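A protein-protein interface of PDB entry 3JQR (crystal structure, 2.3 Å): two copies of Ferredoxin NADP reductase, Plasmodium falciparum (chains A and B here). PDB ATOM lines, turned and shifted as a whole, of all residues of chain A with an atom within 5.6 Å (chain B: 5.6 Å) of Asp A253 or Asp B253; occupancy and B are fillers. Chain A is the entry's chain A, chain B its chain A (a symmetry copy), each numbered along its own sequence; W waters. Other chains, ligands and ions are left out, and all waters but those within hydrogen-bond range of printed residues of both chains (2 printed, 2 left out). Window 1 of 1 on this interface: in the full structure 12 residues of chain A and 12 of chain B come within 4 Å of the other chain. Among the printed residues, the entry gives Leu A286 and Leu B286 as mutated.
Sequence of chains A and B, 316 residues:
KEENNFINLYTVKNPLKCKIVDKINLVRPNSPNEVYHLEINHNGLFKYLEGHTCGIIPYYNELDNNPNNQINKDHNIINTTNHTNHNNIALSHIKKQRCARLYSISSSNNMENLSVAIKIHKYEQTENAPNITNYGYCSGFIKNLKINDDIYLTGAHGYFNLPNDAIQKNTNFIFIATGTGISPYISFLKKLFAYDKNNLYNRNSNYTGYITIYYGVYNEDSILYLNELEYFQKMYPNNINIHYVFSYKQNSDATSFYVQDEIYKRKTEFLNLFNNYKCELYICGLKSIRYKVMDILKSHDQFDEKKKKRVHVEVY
Asp A253 touches Ser B288, and with the chains exchanged Ser A288 touches Asp B253. Ala A254 touches Tyr B291, and with the chains exchanged Tyr A291 touches Ala B254. Phe A257 touches Tyr B291, and with the chains exchanged Tyr A291 touches Phe B257. Phe A257 touches Lys B292, and with the chains exchanged Lys A292 touches Phe B257. Of the 17 pairs that touch across the chains among the printed residues, 17 have their exchanged pair printed and touching as well.
The side-chain amino group (NZ) of Lys A287 lies close to the side-chain amino group (NZ) of Lys B287, 3.1 Å away. The side-chain amino group (NZ) of Lys A292 is in salt-bridge range of the side-chain carboxylate (OD2) of Asp B253 (3.2 Å). OD2 of Asp A253 is in salt-bridge range of NZ of Lys B292 (3.2 Å).
Of the 12 printed residues of chain A, 8 touch a printed residue of chain B. Printed residues of chain A that touch a printed residue of chain B: Asn A251, Asp A253, Ala A254, Phe A257, Lys A287, Ser A288, Tyr A291 and Lys A292. Hydrophobic or aromatic side chains of chain A within 4 Å of the printed part of chain B: Ala A254, Phe A257 and Tyr A291. Of the 12 printed residues of chain B, 8 touch a printed residue of chain A. Hydrophobic or aromatic side chains of chain B within 4 Å of the printed part of chain A: Ala B254, Phe B257 and Tyr B291. Among the printed residues, 17 pairs touch across the chains. Among the printed residues, Asp or Glu carboxylates within 4 Å of a Lys or Arg side-chain nitrogen of the other chain: Asp A253 with Lys B292 (3.2 Å) and Lys A292 with Asp B253 (3.2 Å).
Asn A251 touches Tyr B291. Asp A253 touches Asp B253 (OD1 to OD1, 3.7 Å). Asp A253 touches Ser B288. Asp A253 touches Tyr B291 (OD2 to CD2, 3.3 Å). CB of Ala A254 touches CZ of Tyr B291 (3.6 Å). CZ of Phe B257 touches CZ of Phe A257, at 3.5 Å. CE2 of Tyr B291 touches CE1 of Phe A257, 3.9 Å away. Asp B253 touches Tyr A291 (OD2 to CD2, 3.3 Å). Tyr A291 touches Phe B257. Phe B257 touches Lys A292.
Of chain B, only Asp B253 (3.7 Å), Ser B288 (3.9 Å), Tyr B291 (3.3 Å) and Lys B292 (3.2 Å) come within 4 Å of Asp A253. Of the printed residues of chain A, Tyr B291 touches Asn A251, Asp A253, Ala A254 and Phe A257. Printed residues of chain A within 4 Å of Ser B288: Asp A253. Of the printed residues of chain A, Ala B254 touches Tyr A291 (3.6 Å). Printed residues of chain B within 4 Å of Ala A254: Tyr B291 (3.6 Å). Of the printed residues of chain B, Lys A287 touches Lys B287. Ser B256 touches none of the printed residues of chain A. Ser A252 touches none of the printed residues of chain B. The nearest residue of chain A that does not touch Asp B253 is Lys A287 (5.4 Å). The nearest printed residue of chain A that does not touch Asn B251 is Lys A287 (5.8 Å).
Water W1 lies within hydrogen-bond range of O of Lys A287 (2.6 Å) and OD1 of Asn B251 (3.3 Å). Water W2 bridges the backbone carbonyl oxygen (O) of Lys B287 (2.6 Å) and the side-chain amide oxygen (OD1) of Asn A251 (3.2 Å).
OG1 of Thr A255 lies within hydrogen-bond range of O of Asn A251 (3.4 Å). The side-chain hydroxyl of Ser B256 lies within hydrogen-bond range of the backbone carbonyl oxygen of Asp B253. The side-chain amide nitrogen (ND2) of Asn A251 lies close to the backbone NH (N) of Ala A254 (3.0 Å). The side-chain carboxylate (OD1) of Asp B253 is in salt-bridge range of the side-chain amino group (NZ) of Lys B292, 2.7 Å away. The side-chain amide nitrogen of Asn A251 sits close to the backbone NH of Asp A253. The backbone carbonyl oxygen of Asn B251 lies within hydrogen-bond range of the side-chain hydroxyl of Thr B255 (3.4 Å).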
ATOM      1  N   ASN A 251      23.992  18.679  12.354  1.00  0.00           N
ATOM      2  CA  ASN A 251      22.783  19.449  12.601  1.00  0.00           C
ATOM      3  C   ASN A 251      22.302  19.247  14.036  1.00  0.00           C
ATOM      4  O   ASN A 251      22.280  18.121  14.535  1.00  0.00           O
ATOM      5  CB  ASN A 251      21.694  19.033  11.615  1.00  0.00           C
ATOM      6  CG  ASN A 251      20.412  19.805  11.806  1.00  0.00           C
ATOM      7  OD1 ASN A 251      20.295  20.953  11.379  1.00  0.00           O
ATOM      8  ND2 ASN A 251      19.434  19.174  12.445  1.00  0.00           N
ATOM      9  N   SER A 252      21.910  20.332  14.697  1.00  0.00           N
ATOM     10  CA  SER A 252      21.557  20.275  16.114  1.00  0.00           C
ATOM     11  C   SER A 252      20.146  19.737  16.370  1.00  0.00           C
ATOM     12  O   SER A 252      19.894  19.111  17.399  1.00  0.00           O
ATOM     13  CB  SER A 252      21.720  21.649  16.768  1.00  0.00           C
ATOM     14  OG  SER A 252      20.542  22.422  16.616  1.00  0.00           O
ATOM     15  N   ASP A 253      19.225  19.989  15.446  1.00  0.00           N
ATOM     16  CA  ASP A 253      17.863  19.485  15.589  1.00  0.00           C
ATOM     17  C   ASP A 253      17.870  17.960  15.566  1.00  0.00           C
ATOM     18  O   ASP A 253      17.107  17.313  16.283  1.00  0.00           O
ATOM     19  CB  ASP A 253      16.960  20.027  14.481  1.00  0.00           C
ATOM     20  CG  ASP A 253      15.517  19.572  14.628  1.00  0.00           C
ATOM     21  OD1 ASP A 253      15.021  19.517  15.775  1.00  0.00           O
ATOM     22  OD2 ASP A 253      14.880  19.272  13.593  1.00  0.00           O
ATOM     23  N   ALA A 254      18.742  17.397  14.737  1.00  0.00           N
ATOM     24  CA  ALA A 254      18.892  15.951  14.652  1.00  0.00           C
ATOM     25  C   ALA A 254      19.466  15.384  15.949  1.00  0.00           C
ATOM     26  O   ALA A 254      18.987  14.373  16.460  1.00  0.00           O
ATOM     27  CB  ALA A 254      19.774  15.578  13.468  1.00  0.00           C
ATOM     28  N   THR A 255      20.490  16.047  16.477  1.00  0.00           N
ATOM     29  CA  THR A 255      21.122  15.622  17.722  1.00  0.00           C
ATOM     30  C   THR A 255      20.119  15.520  18.874  1.00  0.00           C
ATOM     31  O   THR A 255      20.198  14.606  19.694  1.00  0.00           O
ATOM     32  CB  THR A 255      22.274  16.568  18.125  1.00  0.00           C
ATOM     33  OG1 THR A 255      23.367  16.405  17.212  1.00  0.00           O
ATOM     34  CG2 THR A 255      22.751  16.259  19.535  1.00  0.00           C
ATOM     35  N   SER A 256      19.179  16.458  18.929  1.00  0.00           N
ATOM     36  CA  SER A 256      18.185  16.480  19.999  1.00  0.00           C
ATOM     37  C   SER A 256      17.167  15.346  19.860  1.00  0.00           C
ATOM     38  O   SER A 256      16.514  14.969  20.832  1.00  0.00           O
ATOM     39  CB  SER A 256      17.473  17.834  20.059  1.00  0.00           C
ATOM     40  OG  SER A 256      16.651  18.034  18.923  1.00  0.00           O
ATOM     41  N   PHE A 257      17.028  14.813  18.648  1.00  0.00           N
ATOM     42  CA  PHE A 257      16.195  13.635  18.425  1.00  0.00           C
ATOM     43  C   PHE A 257      16.867  12.423  19.050  1.00  0.00           C
ATOM     44  O   PHE A 257      16.223  11.612  19.717  1.00  0.00           O
ATOM     45  CB  PHE A 257      15.985  13.379  16.930  1.00  0.00           C
ATOM     46  CG  PHE A 257      14.824  14.129  16.332  1.00  0.00           C
ATOM     47  CD1 PHE A 257      15.039  15.161  15.433  1.00  0.00           C
ATOM     48  CD2 PHE A 257      13.519  13.792  16.659  1.00  0.00           C
ATOM     49  CE1 PHE A 257      13.976  15.851  14.876  1.00  0.00           C
ATOM     50  CE2 PHE A 257      12.450  14.479  16.105  1.00  0.00           C
ATOM     51  CZ  PHE A 257      12.680  15.510  15.213  1.00  0.00           C
ATOM     52  N   LEU A 286      21.185  23.393  24.084  1.00  0.00           N
ATOM     53  CA  LEU A 286      20.595  23.428  22.752  1.00  0.00           C
ATOM     54  C   LEU A 286      19.139  23.869  22.767  1.00  0.00           C
ATOM     55  O   LEU A 286      18.354  23.447  23.615  1.00  0.00           O
ATOM     56  CB  LEU A 286      20.719  22.059  22.078  1.00  0.00           C
ATOM     57  CG  LEU A 286      20.077  21.925  20.695  1.00  0.00           C
ATOM     58  CD1 LEU A 286      20.748  22.859  19.699  1.00  0.00           C
ATOM     59  CD2 LEU A 286      20.142  20.483  20.212  1.00  0.00           C
ATOM     60  N   LYS A 287      18.791  24.723  21.810  1.00  0.00           N
ATOM     61  CA  LYS A 287      17.430  25.217  21.668  1.00  0.00           C
ATOM     62  C   LYS A 287      16.453  24.097  21.329  1.00  0.00           C
ATOM     63  O   LYS A 287      15.327  24.072  21.826  1.00  0.00           O
ATOM     64  CB  LYS A 287      17.366  26.310  20.600  1.00  0.00           C
ATOM     65  CG  LYS A 287      18.103  27.586  20.973  1.00  0.00           C
ATOM     66  CD  LYS A 287      18.020  28.617  19.859  1.00  0.00           C
ATOM     67  CE  LYS A 287      18.735  29.903  20.243  1.00  0.00           C
ATOM     68  NZ  LYS A 287      18.684  30.914  19.152  1.00  0.00           N
ATOM     69  N   SER A 288      16.885  23.179  20.469  1.00  0.00           N
ATOM     70  CA  SER A 288      16.006  22.110  19.999  1.00  0.00           C
ATOM     71  C   SER A 288      15.893  20.939  20.977  1.00  0.00           C
ATOM     72  O   SER A 288      15.206  19.956  20.696  1.00  0.00           O
ATOM     73  CB  SER A 288      16.465  21.606  18.626  1.00  0.00           C
ATOM     74  OG  SER A 288      17.739  20.991  18.705  1.00  0.00           O
ATOM     75  N   TYR A 291      12.002  21.395  24.222  1.00  0.00           N
ATOM     76  CA  TYR A 291      10.681  20.826  23.962  1.00  0.00           C
ATOM     77  C   TYR A 291      10.684  19.298  23.932  1.00  0.00           C
ATOM     78  O   TYR A 291       9.810  18.656  24.515  1.00  0.00           O
ATOM     79  CB  TYR A 291      10.125  21.377  22.645  1.00  0.00           C
ATOM     80  CG  TYR A 291       8.860  20.701  22.168  1.00  0.00           C
ATOM     81  CD1 TYR A 291       7.640  20.951  22.784  1.00  0.00           C
ATOM     82  CD2 TYR A 291       8.884  19.820  21.092  1.00  0.00           C
ATOM     83  CE1 TYR A 291       6.479  20.337  22.349  1.00  0.00           C
ATOM     84  CE2 TYR A 291       7.729  19.201  20.651  1.00  0.00           C
ATOM     85  CZ  TYR A 291       6.530  19.464  21.282  1.00  0.00           C
ATOM     86  OH  TYR A 291       5.379  18.851  20.845  1.00  0.00           O
ATOM     87  N   LYS A 292      11.671  18.724  23.252  1.00  0.00           N
ATOM     88  CA  LYS A 292      11.745  17.278  23.070  1.00  0.00           C
ATOM     89  C   LYS A 292      11.871  16.519  24.393  1.00  0.00           C
ATOM     90  O   LYS A 292      11.365  15.404  24.527  1.00  0.00           O
ATOM     91  CB  LYS A 292      12.902  16.918  22.134  1.00  0.00           C
ATOM     92  CG  LYS A 292      12.760  17.483  20.729  1.00  0.00           C
ATOM     93  CD  LYS A 292      13.757  16.839  19.780  1.00  0.00           C
ATOM     94  CE  LYS A 292      13.521  17.263  18.342  1.00  0.00           C
ATOM     95  NZ  LYS A 292      14.004  18.648  18.074  1.00  0.00           N
ATOM     96  N   ASN B 251       5.800  27.283  21.229  1.00  0.00           N
ATOM     97  CA  ASN B 251       7.140  26.764  21.008  1.00  0.00           C
ATOM     98  C   ASN B 251       7.375  26.498  19.523  1.00  0.00           C
ATOM     99  O   ASN B 251       6.513  25.939  18.845  1.00  0.00           O
ATOM    100  CB  ASN B 251       7.337  25.482  21.814  1.00  0.00           C
ATOM    101  CG  ASN B 251       8.717  24.896  21.642  1.00  0.00           C
ATOM    102  OD1 ASN B 251       9.683  25.366  22.242  1.00  0.00           O
ATOM    103  ND2 ASN B 251       8.817  23.854  20.825  1.00  0.00           N
ATOM    104  N   SER B 252       8.542  26.889  19.021  1.00  0.00           N
ATOM    105  CA  SER B 252       8.821  26.804  17.588  1.00  0.00           C
ATOM    106  C   SER B 252       9.211  25.397  17.125  1.00  0.00           C
ATOM    107  O   SER B 252       8.934  25.015  15.988  1.00  0.00           O
ATOM    108  CB  SER B 252       9.905  27.806  17.187  1.00  0.00           C
ATOM    109  OG  SER B 252      11.196  27.248  17.362  1.00  0.00           O
ATOM    110  N   ASP B 253       9.862  24.632  17.994  1.00  0.00           N
ATOM    111  CA  ASP B 253      10.242  23.266  17.651  1.00  0.00           C
ATOM    112  C   ASP B 253       8.993  22.423  17.422  1.00  0.00           C
ATOM    113  O   ASP B 253       8.963  21.561  16.544  1.00  0.00           O
ATOM    114  CB  ASP B 253      11.105  22.646  18.751  1.00  0.00           C
ATOM    115  CG  ASP B 253      11.571  21.241  18.406  1.00  0.00           C
ATOM    116  OD1 ASP B 253      11.909  20.995  17.227  1.00  0.00           O
ATOM    117  OD2 ASP B 253      11.600  20.383  19.317  1.00  0.00           O
ATOM    118  N   ALA B 254       7.962  22.685  18.219  1.00  0.00           N
ATOM    119  CA  ALA B 254       6.689  21.992  18.076  1.00  0.00           C
ATOM    120  C   ALA B 254       6.012  22.361  16.758  1.00  0.00           C
ATOM    121  O   ALA B 254       5.505  21.495  16.047  1.00  0.00           O
ATOM    122  CB  ALA B 254       5.778  22.309  19.254  1.00  0.00           C
ATOM    123  N   THR B 255       6.013  23.651  16.438  1.00  0.00           N
ATOM    124  CA  THR B 255       5.413  24.137  15.199  1.00  0.00           C
ATOM    125  C   THR B 255       6.004  23.454  13.964  1.00  0.00           C
ATOM    126  O   THR B 255       5.284  23.147  13.013  1.00  0.00           O
ATOM    127  CB  THR B 255       5.561  25.668  15.061  1.00  0.00           C
ATOM    128  OG1 THR B 255       4.724  26.319  16.026  1.00  0.00           O
ATOM    129  CG2 THR B 255       5.159  26.119  13.666  1.00  0.00           C
ATOM    130  N   SER B 256       7.311  23.216  13.984  1.00  0.00           N
ATOM    131  CA  SER B 256       7.990  22.593  12.849  1.00  0.00           C
ATOM    132  C   SER B 256       7.635  21.112  12.710  1.00  0.00           C
ATOM    133  O   SER B 256       7.786  20.532  11.635  1.00  0.00           O
ATOM    134  CB  SER B 256       9.507  22.773  12.953  1.00  0.00           C
ATOM    135  OG  SER B 256      10.041  22.025  14.031  1.00  0.00           O
ATOM    136  N   PHE B 257       7.174  20.503  13.800  1.00  0.00           N
ATOM    137  CA  PHE B 257       6.671  19.133  13.751  1.00  0.00           C
ATOM    138  C   PHE B 257       5.351  19.114  12.995  1.00  0.00           C
ATOM    139  O   PHE B 257       5.116  18.250  12.149  1.00  0.00           O
ATOM    140  CB  PHE B 257       6.451  18.572  15.160  1.00  0.00           C
ATOM    141  CG  PHE B 257       7.675  17.941  15.770  1.00  0.00           C
ATOM    142  CD1 PHE B 257       8.316  18.540  16.843  1.00  0.00           C
ATOM    143  CD2 PHE B 257       8.174  16.745  15.280  1.00  0.00           C
ATOM    144  CE1 PHE B 257       9.438  17.963  17.412  1.00  0.00           C
ATOM    145  CE2 PHE B 257       9.298  16.162  15.845  1.00  0.00           C
ATOM    146  CZ  PHE B 257       9.930  16.772  16.912  1.00  0.00           C
ATOM    147  N   LEU B 286      12.270  29.548  10.243  1.00  0.00           N
ATOM    148  CA  LEU B 286      12.520  28.866  11.506  1.00  0.00           C
ATOM    149  C   LEU B 286      13.714  27.924  11.437  1.00  0.00           C
ATOM    150  O   LEU B 286      13.892  27.191  10.466  1.00  0.00           O
ATOM    151  CB  LEU B 286      11.274  28.096  11.951  1.00  0.00           C
ATOM    152  CG  LEU B 286      11.411  27.270  13.232  1.00  0.00           C
ATOM    153  CD1 LEU B 286      11.703  28.169  14.424  1.00  0.00           C
ATOM    154  CD2 LEU B 286      10.156  26.444  13.474  1.00  0.00           C
ATOM    155  N   LYS B 287      14.526  27.955  12.488  1.00  0.00           N
ATOM    156  CA  LYS B 287      15.695  27.095  12.591  1.00  0.00           C
ATOM    157  C   LYS B 287      15.310  25.621  12.654  1.00  0.00           C
ATOM    158  O   LYS B 287      15.976  24.772  12.064  1.00  0.00           O
ATOM    159  CB  LYS B 287      16.530  27.472  13.816  1.00  0.00           C
ATOM    160  CG  LYS B 287      17.183  28.842  13.725  1.00  0.00           C
ATOM    161  CD  LYS B 287      17.974  29.161  14.983  1.00  0.00           C
ATOM    162  CE  LYS B 287      18.648  30.520  14.881  1.00  0.00           C
ATOM    163  NZ  LYS B 287      19.407  30.858  16.116  1.00  0.00           N
ATOM    164  N   SER B 288      14.239  25.323  13.384  1.00  0.00           N
ATOM    165  CA  SER B 288      13.829  23.936  13.593  1.00  0.00           C
ATOM    166  C   SER B 288      13.023  23.356  12.428  1.00  0.00           C
ATOM    167  O   SER B 288      12.590  22.204  12.481  1.00  0.00           O
ATOM    168  CB  SER B 288      13.036  23.803  14.898  1.00  0.00           C
ATOM    169  OG  SER B 288      11.813  24.515  14.830  1.00  0.00           O
ATOM    170  N   TYR B 291      15.903  20.973   8.977  1.00  0.00           N
ATOM    171  CA  TYR B 291      16.170  19.536   9.024  1.00  0.00           C
ATOM    172  C   TYR B 291      14.920  18.687   8.801  1.00  0.00           C
ATOM    173  O   TYR B 291      14.946  17.715   8.046  1.00  0.00           O
ATOM    174  CB  TYR B 291      16.824  19.170  10.361  1.00  0.00           C
ATOM    175  CG  TYR B 291      16.954  17.684  10.608  1.00  0.00           C
ATOM    176  CD1 TYR B 291      17.909  16.930   9.938  1.00  0.00           C
ATOM    177  CD2 TYR B 291      16.128  17.037  11.520  1.00  0.00           C
ATOM    178  CE1 TYR B 291      18.034  15.570  10.162  1.00  0.00           C
ATOM    179  CE2 TYR B 291      16.245  15.679  11.751  1.00  0.00           C
ATOM    180  CZ  TYR B 291      17.199  14.951  11.070  1.00  0.00           C
ATOM    181  OH  TYR B 291      17.320  13.600  11.298  1.00  0.00           O
ATOM    182  N   LYS B 292      13.828  19.062   9.460  1.00  0.00           N
ATOM    183  CA  LYS B 292      12.590  18.291   9.405  1.00  0.00           C
ATOM    184  C   LYS B 292      12.014  18.192   7.990  1.00  0.00           C
ATOM    185  O   LYS B 292      11.406  17.184   7.630  1.00  0.00           O
ATOM    186  CB  LYS B 292      11.554  18.880  10.365  1.00  0.00           C
ATOM    187  CG  LYS B 292      11.974  18.845  11.827  1.00  0.00           C
ATOM    188  CD  LYS B 292      10.796  19.144  12.739  1.00  0.00           C
ATOM    189  CE  LYS B 292      11.152  18.948  14.201  1.00  0.00           C
ATOM    190  NZ  LYS B 292      11.982  20.065  14.736  1.00  0.00           N
HETATM  191  O   HOH W   1      12.816  24.501  22.304  1.00  0.00           O
HETATM  192  O   HOH W   2      17.804  23.039  11.447  1.00  0.00           O
